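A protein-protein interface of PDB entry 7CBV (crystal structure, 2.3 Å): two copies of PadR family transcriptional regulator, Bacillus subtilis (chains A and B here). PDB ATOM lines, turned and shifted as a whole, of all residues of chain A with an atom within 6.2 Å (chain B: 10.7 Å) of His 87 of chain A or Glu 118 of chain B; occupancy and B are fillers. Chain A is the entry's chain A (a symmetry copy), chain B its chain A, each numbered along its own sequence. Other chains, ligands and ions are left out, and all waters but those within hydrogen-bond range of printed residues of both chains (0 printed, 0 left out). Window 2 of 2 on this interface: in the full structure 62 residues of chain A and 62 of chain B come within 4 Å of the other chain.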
ATOM      1  N   GLY A  82      27.742 -17.533  22.572  1.00  0.00           N
ATOM      2  CA  GLY A  82      26.388 -17.868  22.978  1.00  0.00           C
ATOM      3  C   GLY A  82      25.486 -16.654  23.007  1.00  0.00           C
ATOM      4  O   GLY A  82      24.322 -16.722  22.604  1.00  0.00           O
ATOM      5  N   LYS A  83      26.016 -15.523  23.481  1.00  0.00           N
ATOM      6  CA  LYS A  83      25.253 -14.280  23.454  1.00  0.00           C
ATOM      7  C   LYS A  83      24.850 -13.921  22.029  1.00  0.00           C
ATOM      8  O   LYS A  83      23.687 -13.581  21.767  1.00  0.00           O
ATOM      9  CB  LYS A  83      26.070 -13.158  24.086  1.00  0.00           C
ATOM     10  CG  LYS A  83      25.292 -11.870  24.317  1.00  0.00           C
ATOM     11  CD  LYS A  83      26.115 -10.789  25.031  1.00  0.00           C
ATOM     12  CE  LYS A  83      25.276  -9.508  25.159  1.00  0.00           C
ATOM     13  NZ  LYS A  83      25.943  -8.464  25.962  1.00  0.00           N
ATOM     14  N   GLN A  84      25.788 -14.039  21.090  1.00  0.00           N
ATOM     15  CA  GLN A  84      25.496 -13.713  19.695  1.00  0.00           C
ATOM     16  C   GLN A  84      24.486 -14.680  19.104  1.00  0.00           C
ATOM     17  O   GLN A  84      23.578 -14.271  18.368  1.00  0.00           O
ATOM     18  CB  GLN A  84      26.775 -13.735  18.859  1.00  0.00           C
ATOM     19  CG  GLN A  84      26.536 -13.287  17.440  1.00  0.00           C
ATOM     20  CD  GLN A  84      26.201 -11.800  17.407  1.00  0.00           C
ATOM     21  OE1 GLN A  84      26.863 -10.992  18.084  1.00  0.00           O
ATOM     22  NE2 GLN A  84      25.151 -11.432  16.665  1.00  0.00           N
ATOM     23  N   GLU A  85      24.616 -15.962  19.444  1.00  0.00           N
ATOM     24  CA  GLU A  85      23.694 -16.976  18.936  1.00  0.00           C
ATOM     25  C   GLU A  85      22.284 -16.695  19.427  1.00  0.00           C
ATOM     26  O   GLU A  85      21.320 -16.749  18.654  1.00  0.00           O
ATOM     27  CB  GLU A  85      24.171 -18.353  19.411  1.00  0.00           C
ATOM     28  CG  GLU A  85      23.424 -19.529  18.861  1.00  0.00           C
ATOM     29  CD  GLU A  85      23.842 -19.861  17.446  1.00  0.00           C
ATOM     30  OE1 GLU A  85      24.658 -19.112  16.851  1.00  0.00           O
ATOM     31  OE2 GLU A  85      23.352 -20.882  16.938  1.00  0.00           O
ATOM     32  N   LEU A  86      22.163 -16.362  20.714  1.00  0.00           N
ATOM     33  CA  LEU A  86      20.890 -15.955  21.293  1.00  0.00           C
ATOM     34  C   LEU A  86      20.335 -14.728  20.584  1.00  0.00           C
ATOM     35  O   LEU A  86      19.148 -14.677  20.240  1.00  0.00           O
ATOM     36  CB  LEU A  86      21.074 -15.677  22.789  1.00  0.00           C
ATOM     37  CG  LEU A  86      19.844 -15.105  23.510  1.00  0.00           C
ATOM     38  CD1 LEU A  86      18.673 -16.125  23.467  1.00  0.00           C
ATOM     39  CD2 LEU A  86      20.160 -14.652  24.958  1.00  0.00           C
ATOM     40  N   HIS A  87      21.185 -13.727  20.362  1.00  0.00           N
ATOM     41  CA  HIS A  87      20.740 -12.484  19.728  1.00  0.00           C
ATOM     42  C   HIS A  87      20.222 -12.728  18.320  1.00  0.00           C
ATOM     43  O   HIS A  87      19.158 -12.220  17.949  1.00  0.00           O
ATOM     44  CB  HIS A  87      21.893 -11.481  19.692  1.00  0.00           C
ATOM     45  CG  HIS A  87      21.579 -10.224  18.946  1.00  0.00           C
ATOM     46  ND1 HIS A  87      20.861  -9.181  19.495  1.00  0.00           N
ATOM     47  CD2 HIS A  87      21.867  -9.858  17.673  1.00  0.00           C
ATOM     48  CE1 HIS A  87      20.732  -8.223  18.595  1.00  0.00           C
ATOM     49  NE2 HIS A  87      21.341  -8.605  17.484  1.00  0.00           N
ATOM     50  N   ASP A  88      20.968 -13.501  17.512  1.00  0.00           N
ATOM     51  CA  ASP A  88      20.524 -13.795  16.146  1.00  0.00           C
ATOM     52  C   ASP A  88      19.157 -14.467  16.130  1.00  0.00           C
ATOM     53  O   ASP A  88      18.332 -14.200  15.242  1.00  0.00           O
ATOM     54  CB  ASP A  88      21.546 -14.676  15.415  1.00  0.00           C
ATOM     55  CG  ASP A  88      22.892 -13.978  15.216  1.00  0.00           C
ATOM     56  OD1 ASP A  88      22.959 -12.740  15.355  1.00  0.00           O
ATOM     57  OD2 ASP A  88      23.876 -14.671  14.876  1.00  0.00           O
ATOM     58  N   TRP A  89      18.913 -15.379  17.077  1.00  0.00           N
ATOM     59  CA  TRP A  89      17.617 -16.063  17.143  1.00  0.00           C
ATOM     60  C   TRP A  89      16.499 -15.114  17.571  1.00  0.00           C
ATOM     61  O   TRP A  89      15.382 -15.176  17.038  1.00  0.00           O
ATOM     62  CB  TRP A  89      17.725 -17.256  18.098  1.00  0.00           C
ATOM     63  CG  TRP A  89      16.429 -17.927  18.448  1.00  0.00           C
ATOM     64  CD1 TRP A  89      15.733 -18.838  17.685  1.00  0.00           C
ATOM     65  CD2 TRP A  89      15.692 -17.778  19.661  1.00  0.00           C
ATOM     66  NE1 TRP A  89      14.599 -19.236  18.349  1.00  0.00           N
ATOM     67  CE2 TRP A  89      14.553 -18.606  19.566  1.00  0.00           C
ATOM     68  CE3 TRP A  89      15.890 -17.039  20.824  1.00  0.00           C
ATOM     69  CZ2 TRP A  89      13.610 -18.693  20.581  1.00  0.00           C
ATOM     70  CZ3 TRP A  89      14.951 -17.130  21.836  1.00  0.00           C
ATOM     71  CH2 TRP A  89      13.821 -17.948  21.703  1.00  0.00           C
ATOM     72  N   LEU A  90      16.773 -14.249  18.556  1.00  0.00           N
ATOM     73  CA  LEU A  90      15.765 -13.312  19.040  1.00  0.00           C
ATOM     74  C   LEU A  90      15.212 -12.444  17.918  1.00  0.00           C
ATOM     75  O   LEU A  90      13.998 -12.282  17.788  1.00  0.00           O
ATOM     76  CB  LEU A  90      16.356 -12.415  20.129  1.00  0.00           C
ATOM     77  CG  LEU A  90      16.533 -13.103  21.481  1.00  0.00           C
ATOM     78  CD1 LEU A  90      17.368 -12.249  22.404  1.00  0.00           C
ATOM     79  CD2 LEU A  90      15.162 -13.399  22.121  1.00  0.00           C
ATOM     80  N   ILE A  91      16.087 -11.884  17.086  1.00  0.00           N
ATOM     81  CA  ILE A  91      15.627 -10.876  16.136  1.00  0.00           C
ATOM     82  C   ILE A  91      15.148 -11.484  14.840  1.00  0.00           C
ATOM     83  O   ILE A  91      14.662 -10.754  13.966  1.00  0.00           O
ATOM     84  CB  ILE A  91      16.745  -9.868  15.822  1.00  0.00           C
ATOM     85  CG1 ILE A  91      17.887 -10.589  15.103  1.00  0.00           C
ATOM     86  CG2 ILE A  91      17.219  -9.192  17.098  1.00  0.00           C
ATOM     87  CD1 ILE A  91      18.959  -9.662  14.540  1.00  0.00           C
ATOM     88  N   ARG A  92      15.300 -12.786  14.680  1.00  0.00           N
ATOM     89  CA  ARG A  92      14.894 -13.474  13.472  1.00  0.00           C
ATOM     90  C   ARG A  92      13.375 -13.515  13.364  1.00  0.00           C
ATOM     91  O   ARG A  92      12.664 -13.751  14.347  1.00  0.00           O
ATOM     92  CB  ARG A  92      15.529 -14.862  13.479  1.00  0.00           C
ATOM     93  CG  ARG A  92      15.485 -15.665  12.214  1.00  0.00           C
ATOM     94  CD  ARG A  92      16.885 -16.250  12.039  1.00  0.00           C
ATOM     95  NE  ARG A  92      17.274 -17.042  13.206  1.00  0.00           N
ATOM     96  CZ  ARG A  92      18.528 -17.391  13.508  1.00  0.00           C
ATOM     97  NH1 ARG A  92      19.541 -17.018  12.728  1.00  0.00           N
ATOM     98  NH2 ARG A  92      18.768 -18.117  14.595  1.00  0.00           N
ATOM     99  N   PHE B 104       7.649 -17.512  19.949  1.00  0.00           N
ATOM    100  CA  PHE B 104       7.668 -16.055  20.082  1.00  0.00           C
ATOM    101  C   PHE B 104       7.594 -15.638  21.543  1.00  0.00           C
ATOM    102  O   PHE B 104       8.252 -14.683  21.958  1.00  0.00           O
ATOM    103  CB  PHE B 104       6.506 -15.438  19.302  1.00  0.00           C
ATOM    104  CG  PHE B 104       6.375 -13.952  19.490  1.00  0.00           C
ATOM    105  CD1 PHE B 104       7.131 -13.071  18.722  1.00  0.00           C
ATOM    106  CD2 PHE B 104       5.504 -13.440  20.436  1.00  0.00           C
ATOM    107  CE1 PHE B 104       7.018 -11.697  18.899  1.00  0.00           C
ATOM    108  CE2 PHE B 104       5.388 -12.083  20.623  1.00  0.00           C
ATOM    109  CZ  PHE B 104       6.140 -11.197  19.845  1.00  0.00           C
ATOM    110  N   LYS B 107      10.836 -15.824  23.267  1.00  0.00           N
ATOM    111  CA  LYS B 107      11.532 -14.573  22.997  1.00  0.00           C
ATOM    112  C   LYS B 107      11.024 -13.457  23.896  1.00  0.00           C
ATOM    113  O   LYS B 107      11.813 -12.667  24.425  1.00  0.00           O
ATOM    114  CB  LYS B 107      11.361 -14.173  21.527  1.00  0.00           C
ATOM    115  CG  LYS B 107      11.970 -15.138  20.533  1.00  0.00           C
ATOM    116  CD  LYS B 107      11.802 -14.611  19.117  1.00  0.00           C
ATOM    117  CE  LYS B 107      12.367 -15.623  18.134  1.00  0.00           C
ATOM    118  NZ  LYS B 107      12.500 -15.052  16.781  1.00  0.00           N
ATOM    119  N   ALA B 108       9.695 -13.329  24.028  1.00  0.00           N
ATOM    120  CA  ALA B 108       9.161 -12.252  24.857  1.00  0.00           C
ATOM    121  C   ALA B 108       9.673 -12.369  26.280  1.00  0.00           C
ATOM    122  O   ALA B 108       9.972 -11.359  26.924  1.00  0.00           O
ATOM    123  CB  ALA B 108       7.632 -12.236  24.840  1.00  0.00           C
ATOM    124  N   PHE B 110      12.501 -13.363  27.190  1.00  0.00           N
ATOM    125  CA  PHE B 110      13.895 -12.953  27.158  1.00  0.00           C
ATOM    126  C   PHE B 110      14.077 -11.548  26.614  1.00  0.00           C
ATOM    127  O   PHE B 110      15.175 -11.197  26.151  1.00  0.00           O
ATOM    128  CB  PHE B 110      14.712 -13.949  26.334  1.00  0.00           C
ATOM    129  CG  PHE B 110      14.713 -15.358  26.902  1.00  0.00           C
ATOM    130  CD1 PHE B 110      14.847 -15.571  28.261  1.00  0.00           C
ATOM    131  CD2 PHE B 110      14.612 -16.460  26.070  1.00  0.00           C
ATOM    132  CE1 PHE B 110      14.870 -16.864  28.790  1.00  0.00           C
ATOM    133  CE2 PHE B 110      14.658 -17.743  26.587  1.00  0.00           C
ATOM    134  CZ  PHE B 110      14.772 -17.951  27.947  1.00  0.00           C
ATOM    135  N   ILE B 111      13.030 -10.726  26.675  1.00  0.00           N
ATOM    136  CA  ILE B 111      13.062  -9.424  26.014  1.00  0.00           C
ATOM    137  C   ILE B 111      14.159  -8.506  26.563  1.00  0.00           C
ATOM    138  O   ILE B 111      14.545  -7.546  25.891  1.00  0.00           O
ATOM    139  CB  ILE B 111      11.684  -8.760  26.143  1.00  0.00           C
ATOM    140  CG1 ILE B 111      11.614  -7.516  25.250  1.00  0.00           C
ATOM    141  CG2 ILE B 111      11.420  -8.435  27.610  1.00  0.00           C
ATOM    142  CD1 ILE B 111      10.317  -6.790  25.290  1.00  0.00           C
ATOM    143  N   SER B 112      14.697  -8.790  27.761  1.00  0.00           N
ATOM    144  CA  SER B 112      15.740  -7.920  28.309  1.00  0.00           C
ATOM    145  C   SER B 112      17.000  -7.928  27.457  1.00  0.00           C
ATOM    146  O   SER B 112      17.834  -7.026  27.605  1.00  0.00           O
ATOM    147  CB  SER B 112      16.097  -8.311  29.749  1.00  0.00           C
ATOM    148  OG  SER B 112      16.817  -9.536  29.808  1.00  0.00           O
ATOM    149  N   SER B 113      17.150  -8.913  26.567  1.00  0.00           N
ATOM    150  CA  SER B 113      18.262  -8.975  25.622  1.00  0.00           C
ATOM    151  C   SER B 113      18.017  -8.186  24.343  1.00  0.00           C
ATOM    152  O   SER B 113      18.866  -8.223  23.456  1.00  0.00           O
ATOM    153  CB  SER B 113      18.563 -10.430  25.234  1.00  0.00           C
ATOM    154  OG  SER B 113      19.042 -11.161  26.343  1.00  0.00           O
ATOM    155  N   LEU B 114      16.897  -7.470  24.218  1.00  0.00           N
ATOM    156  CA  LEU B 114      16.600  -6.718  23.008  1.00  0.00           C
ATOM    157  C   LEU B 114      16.579  -5.231  23.327  1.00  0.00           C
ATOM    158  O   LEU B 114      16.114  -4.825  24.393  1.00  0.00           O
ATOM    159  CB  LEU B 114      15.232  -7.131  22.400  1.00  0.00           C
ATOM    160  CG  LEU B 114      15.096  -8.538  21.807  1.00  0.00           C
ATOM    161  CD1 LEU B 114      13.742  -8.724  21.204  1.00  0.00           C
ATOM    162  CD2 LEU B 114      16.163  -8.752  20.758  1.00  0.00           C
ATOM    163  N   SER B 115      17.075  -4.423  22.396  1.00  0.00           N
ATOM    164  CA  SER B 115      16.839  -2.995  22.489  1.00  0.00           C
ATOM    165  C   SER B 115      15.349  -2.702  22.305  1.00  0.00           C
ATOM    166  O   SER B 115      14.571  -3.550  21.859  1.00  0.00           O
ATOM    167  CB  SER B 115      17.644  -2.247  21.429  1.00  0.00           C
ATOM    168  OG  SER B 115      17.145  -2.502  20.123  1.00  0.00           O
ATOM    169  N   ARG B 116      14.958  -1.478  22.655  1.00  0.00           N
ATOM    170  CA  ARG B 116      13.581  -1.037  22.430  1.00  0.00           C
ATOM    171  C   ARG B 116      13.200  -1.174  20.957  1.00  0.00           C
ATOM    172  O   ARG B 116      12.130  -1.696  20.621  1.00  0.00           O
ATOM    173  CB  ARG B 116      13.427   0.416  22.891  1.00  0.00           C
ATOM    174  CG  ARG B 116      11.998   0.845  23.214  1.00  0.00           C
ATOM    175  CD  ARG B 116      11.754   2.269  22.702  1.00  0.00           C
ATOM    176  NE  ARG B 116      11.043   2.205  21.425  1.00  0.00           N
ATOM    177  CZ  ARG B 116      11.539   2.555  20.241  1.00  0.00           C
ATOM    178  NH1 ARG B 116      12.768   3.040  20.135  1.00  0.00           N
ATOM    179  NH2 ARG B 116      10.786   2.428  19.153  1.00  0.00           N
ATOM    180  N   GLN B 117      14.088  -0.729  20.067  1.00  0.00           N
ATOM    181  CA  GLN B 117      13.816  -0.776  18.635  1.00  0.00           C
ATOM    182  C   GLN B 117      13.693  -2.213  18.135  1.00  0.00           C
ATOM    183  O   GLN B 117      12.825  -2.514  17.313  1.00  0.00           O
ATOM    184  CB  GLN B 117      14.920  -0.035  17.872  1.00  0.00           C
ATOM    185  CG  GLN B 117      14.636   0.120  16.382  1.00  0.00           C
ATOM    186  CD  GLN B 117      13.342   0.917  16.124  1.00  0.00           C
ATOM    187  OE1 GLN B 117      13.233   2.071  16.523  1.00  0.00           O
ATOM    188  NE2 GLN B 117      12.370   0.296  15.439  1.00  0.00           N
ATOM    189  N   GLU B 118      14.572  -3.105  18.596  1.00  0.00           N
ATOM    190  CA  GLU B 118      14.520  -4.503  18.169  1.00  0.00           C
ATOM    191  C   GLU B 118      13.250  -5.179  18.669  1.00  0.00           C
ATOM    192  O   GLU B 118      12.637  -5.973  17.948  1.00  0.00           O
ATOM    193  CB  GLU B 118      15.750  -5.262  18.687  1.00  0.00           C
ATOM    194  CG  GLU B 118      17.045  -4.884  18.026  1.00  0.00           C
ATOM    195  CD  GLU B 118      18.288  -5.481  18.712  1.00  0.00           C
ATOM    196  OE1 GLU B 118      18.253  -5.814  19.922  1.00  0.00           O
ATOM    197  OE2 GLU B 118      19.317  -5.610  18.024  1.00  0.00           O
ATOM    198  N   ALA B 119      12.851  -4.897  19.911  1.00  0.00           N
ATOM    199  CA  ALA B 119      11.605  -5.459  20.419  1.00  0.00           C
ATOM    200  C   ALA B 119      10.402  -4.911  19.649  1.00  0.00           C
ATOM    201  O   ALA B 119       9.474  -5.658  19.312  1.00  0.00           O
ATOM    202  CB  ALA B 119      11.476  -5.180  21.909  1.00  0.00           C
ATOM    203  N   SER B 120      10.402  -3.606  19.369  1.00  0.00           N
ATOM    204  CA  SER B 120       9.344  -3.025  18.551  1.00  0.00           C
ATOM    205  C   SER B 120       9.273  -3.703  17.186  1.00  0.00           C
ATOM    206  O   SER B 120       8.195  -4.114  16.741  1.00  0.00           O
ATOM    207  CB  SER B 120       9.580  -1.521  18.404  1.00  0.00           C
ATOM    208  OG  SER B 120       8.597  -0.953  17.561  1.00  0.00           O
ATOM    209  N   ASP B 121      10.425  -3.861  16.525  1.00  0.00           N
ATOM    210  CA  ASP B 121      10.472  -4.528  15.220  1.00  0.00           C
ATOM    211  C   ASP B 121       9.964  -5.966  15.309  1.00  0.00           C
ATOM    212  O   ASP B 121       9.224  -6.428  14.437  1.00  0.00           O
ATOM    213  CB  ASP B 121      11.906  -4.512  14.676  1.00  0.00           C
ATOM    214  CG  ASP B 121      12.351  -3.133  14.257  1.00  0.00           C
ATOM    215  OD1 ASP B 121      11.533  -2.188  14.349  1.00  0.00           O
ATOM    216  OD2 ASP B 121      13.526  -2.986  13.859  1.00  0.00           O
ATOM    217  N   LEU B 122      10.385  -6.695  16.338  1.00  0.00           N
ATOM    218  CA  LEU B 122       9.959  -8.081  16.517  1.00  0.00           C
ATOM    219  C   LEU B 122       8.453  -8.174  16.752  1.00  0.00           C
ATOM    220  O   LEU B 122       7.765  -9.031  16.179  1.00  0.00           O
ATOM    221  CB  LEU B 122      10.713  -8.693  17.700  1.00  0.00           C
ATOM    222  CG  LEU B 122      10.381 -10.162  17.989  1.00  0.00           C
ATOM    223  CD1 LEU B 122      10.968 -11.031  16.883  1.00  0.00           C
ATOM    224  CD2 LEU B 122      10.895 -10.575  19.385  1.00  0.00           C
ATOM    225  N   PHE B 123       7.934  -7.329  17.639  1.00  0.00           N
ATOM    226  CA  PHE B 123       6.511  -7.374  17.946  1.00  0.00           C
ATOM    227  C   PHE B 123       5.680  -6.887  16.765  1.00  0.00           C
ATOM    228  O   PHE B 123       4.589  -7.408  16.514  1.00  0.00           O
ATOM    229  CB  PHE B 123       6.227  -6.553  19.214  1.00  0.00           C
ATOM    230  CG  PHE B 123       6.355  -7.355  20.480  1.00  0.00           C
ATOM    231  CD1 PHE B 123       7.585  -7.814  20.906  1.00  0.00           C
ATOM    232  CD2 PHE B 123       5.238  -7.663  21.235  1.00  0.00           C
ATOM    233  CE1 PHE B 123       7.706  -8.583  22.059  1.00  0.00           C
ATOM    234  CE2 PHE B 123       5.355  -8.441  22.395  1.00  0.00           C
ATOM    235  CZ  PHE B 123       6.587  -8.893  22.800  1.00  0.00           C
ATOM    236  N   THR B 124       6.186  -5.898  16.026  1.00  0.00           N
ATOM    237  CA  THR B 124       5.458  -5.373  14.875  1.00  0.00           C
ATOM    238  C   THR B 124       5.340  -6.424  13.787  1.00  0.00           C
ATOM    239  O   THR B 124       4.271  -6.598  13.190  1.00  0.00           O
ATOM    240  CB  THR B 124       6.161  -4.120  14.343  1.00  0.00           C
ATOM    241  OG1 THR B 124       6.170  -3.127  15.368  1.00  0.00           O
ATOM    242  CG2 THR B 124       5.421  -3.536  13.142  1.00  0.00           C
ATOM    243  N   ASP B 125       6.427  -7.141  13.524  1.00  0.00           N
ATOM    244  CA  ASP B 125       6.366  -8.235  12.569  1.00  0.00           C
ATOM    245  C   ASP B 125       5.389  -9.310  13.032  1.00  0.00           C
ATOM    246  O   ASP B 125       4.643  -9.878  12.222  1.00  0.00           O
ATOM    247  CB  ASP B 125       7.755  -8.818  12.356  1.00  0.00           C
ATOM    248  CG  ASP B 125       7.710 -10.118  11.600  1.00  0.00           C
ATOM    249  OD1 ASP B 125       7.518 -10.074  10.371  1.00  0.00           O
ATOM    250  OD2 ASP B 125       7.857 -11.181  12.233  1.00  0.00           O
ATOM    251  N   GLN B 126       5.366  -9.600  14.332  1.00  0.00           N
ATOM    252  CA  GLN B 126       4.417 -10.592  14.818  1.00  0.00           C
ATOM    253  C   GLN B 126       2.980 -10.099  14.653  1.00  0.00           C
ATOM    254  O   GLN B 126       2.116 -10.843  14.179  1.00  0.00           O
ATOM    255  CB  GLN B 126       4.725 -10.923  16.276  1.00  0.00           C
ATOM    256  CG  GLN B 126       3.968 -12.137  16.836  1.00  0.00           C
ATOM    257  CD  GLN B 126       4.452 -13.484  16.316  1.00  0.00           C
ATOM    258  OE1 GLN B 126       3.778 -14.488  16.518  1.00  0.00           O
ATOM    259  NE2 GLN B 126       5.617 -13.513  15.646  1.00  0.00           N
ATOM    260  N   ILE B 181       0.970  -4.406  23.891  1.00  0.00           N
ATOM    261  CA  ILE B 181       2.390  -4.387  24.250  1.00  0.00           C
ATOM    262  C   ILE B 181       3.135  -3.374  23.396  1.00  0.00           C
ATOM    263  O   ILE B 181       3.992  -2.634  23.895  1.00  0.00           O
ATOM    264  CB  ILE B 181       3.019  -5.786  24.148  1.00  0.00           C
ATOM    265  CG1 ILE B 181       2.308  -6.770  25.093  1.00  0.00           C
ATOM    266  CG2 ILE B 181       4.508  -5.687  24.507  1.00  0.00           C
ATOM    267  CD1 ILE B 181       2.145  -6.177  26.531  1.00  0.00           C
ATOM    268  N   LEU B 182       2.819  -3.318  22.098  1.00  0.00           N
ATOM    269  CA  LEU B 182       3.400  -2.292  21.238  1.00  0.00           C
ATOM    270  C   LEU B 182       3.070  -0.894  21.744  1.00  0.00           C
ATOM    271  O   LEU B 182       3.897   0.029  21.636  1.00  0.00           O
ATOM    272  CB  LEU B 182       2.929  -2.476  19.803  1.00  0.00           C
ATOM    273  CG  LEU B 182       3.737  -3.550  19.087  1.00  0.00           C
ATOM    274  CD1 LEU B 182       3.050  -3.950  17.771  1.00  0.00           C
ATOM    275  CD2 LEU B 182       5.113  -2.986  18.819  1.00  0.00           C
ATOM    276  N   ILE B 185       5.596  -0.465  24.461  1.00  0.00           N
ATOM    277  CA  ILE B 185       6.984  -0.406  24.011  1.00  0.00           C
ATOM    278  C   ILE B 185       7.258   0.911  23.296  1.00  0.00           C
ATOM    279  O   ILE B 185       8.264   1.578  23.553  1.00  0.00           O
ATOM    280  CB  ILE B 185       7.288  -1.620  23.117  1.00  0.00           C
ATOM    281  CG1 ILE B 185       7.389  -2.883  23.938  1.00  0.00           C
ATOM    282  CG2 ILE B 185       8.550  -1.466  22.330  1.00  0.00           C
ATOM    283  CD1 ILE B 185       7.602  -4.102  23.046  1.00  0.00           C
ATOM    284  N   ASP B 186       6.364   1.306  22.398  1.00  0.00           N
ATOM    285  CA  ASP B 186       6.509   2.534  21.640  1.00  0.00           C
ATOM    286  C   ASP B 186       5.960   3.717  22.394  1.00  0.00           C
ATOM    287  O   ASP B 186       6.099   4.842  21.930  1.00  0.00           O
ATOM    288  CB  ASP B 186       5.804   2.401  20.293  1.00  0.00           C
ATOM    289  CG  ASP B 186       6.417   1.318  19.414  1.00  0.00           C
ATOM    290  OD1 ASP B 186       7.645   1.092  19.512  1.00  0.00           O
ATOM    291  OD2 ASP B 186       5.658   0.669  18.653  1.00  0.00           O
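The side-chain amino group of Lys 107 of chain B lies within hydrogen-bond range of the backbone carbonyl oxygen of Trp 89 of chain A, at 2.9 Å. The side-chain amino group (NZ) of Lys 107 of chain B sits at hydrogen-bond distance from the backbone carbonyl oxygen (O) of Leu 90 of chain A (3.3 Å). The side-chain amino group (NZ) of Lys 107 of chain B sits at hydrogen-bond distance from the backbone carbonyl oxygen (O) of Arg 92 of chain A.
OG of Ser 115 of chain B is in hydrogen-bond range of N of Glu 118 of chain B, at 3.1 Å.
Among the printed residues, merely in contact across the chains: His 87 of chain A with Glu 118 of chain B, Leu 90 of chain A with Leu 122 of chain B, Leu 90 of chain A with Ser 113 of chain B, Leu 90 of chain A with Leu 114 of chain B, Ile 91 of chain A with Leu 114 of chain B and Leu 86 of chain A with Ser 113 of chain B.
His 87 of chain A touches just one residue of chain B: Glu 118 (3.0 Å). Glu 118 of chain B touches just one residue of chain A: His 87. No residue of chain B comes within 4 Å of Gln 84 of chain A. No residue of chain B comes within 4 Å of Asp 88 of chain A. Printed residues of chain B within 4 Å of Leu 90 of chain A: Lys 107 (3.3 Å), Ser 113 (3.6 Å), Leu 114 (3.7 Å) and Leu 122 (3.4 Å). Of chain B, only Leu 114 comes within 4 Å of Ile 91 of chain A. Printed residues of chain A within 4 Å of Lys 107 of chain B: Trp 89 (2.9 Å), Leu 90 (3.3 Å) and Arg 92 (2.8 Å). Of the printed residues of chain B, Arg 92 of chain A touches Lys 107. Printed residues of chain A within 4 Å of Leu 114 of chain B: Leu 90 (3.7 Å) and Ile 91 (3.8 Å). Of the printed residues of chain A, Leu 122 of chain B touches Leu 90. Printed residues of chain A within 4 Å of Ser 113 of chain B: Leu 86 (3.9 Å) and Leu 90 (3.6 Å). Phe 104 of chain B touches none of the printed residues of chain A. The nearest printed residue of chain A that does not touch Leu 114 of chain B is His 87 of chain A (4.9 Å).
Of the 24 printed residues of chain B, 5 touch a printed residue of chain A. Along chain B the printed residues that touch a printed residue of chain A span positions 107 to 122. Hydrophobic or aromatic side chains of chain A within 4 Å of the printed part of chain B: Leu 86, His 87, Trp 89, Leu 90 and Ile 91. Among the printed residues, no Asp or Glu carboxylate lies within 4 Å of a Lys or Arg side-chain nitrogen of the other chain.
No position is printed for both chains.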
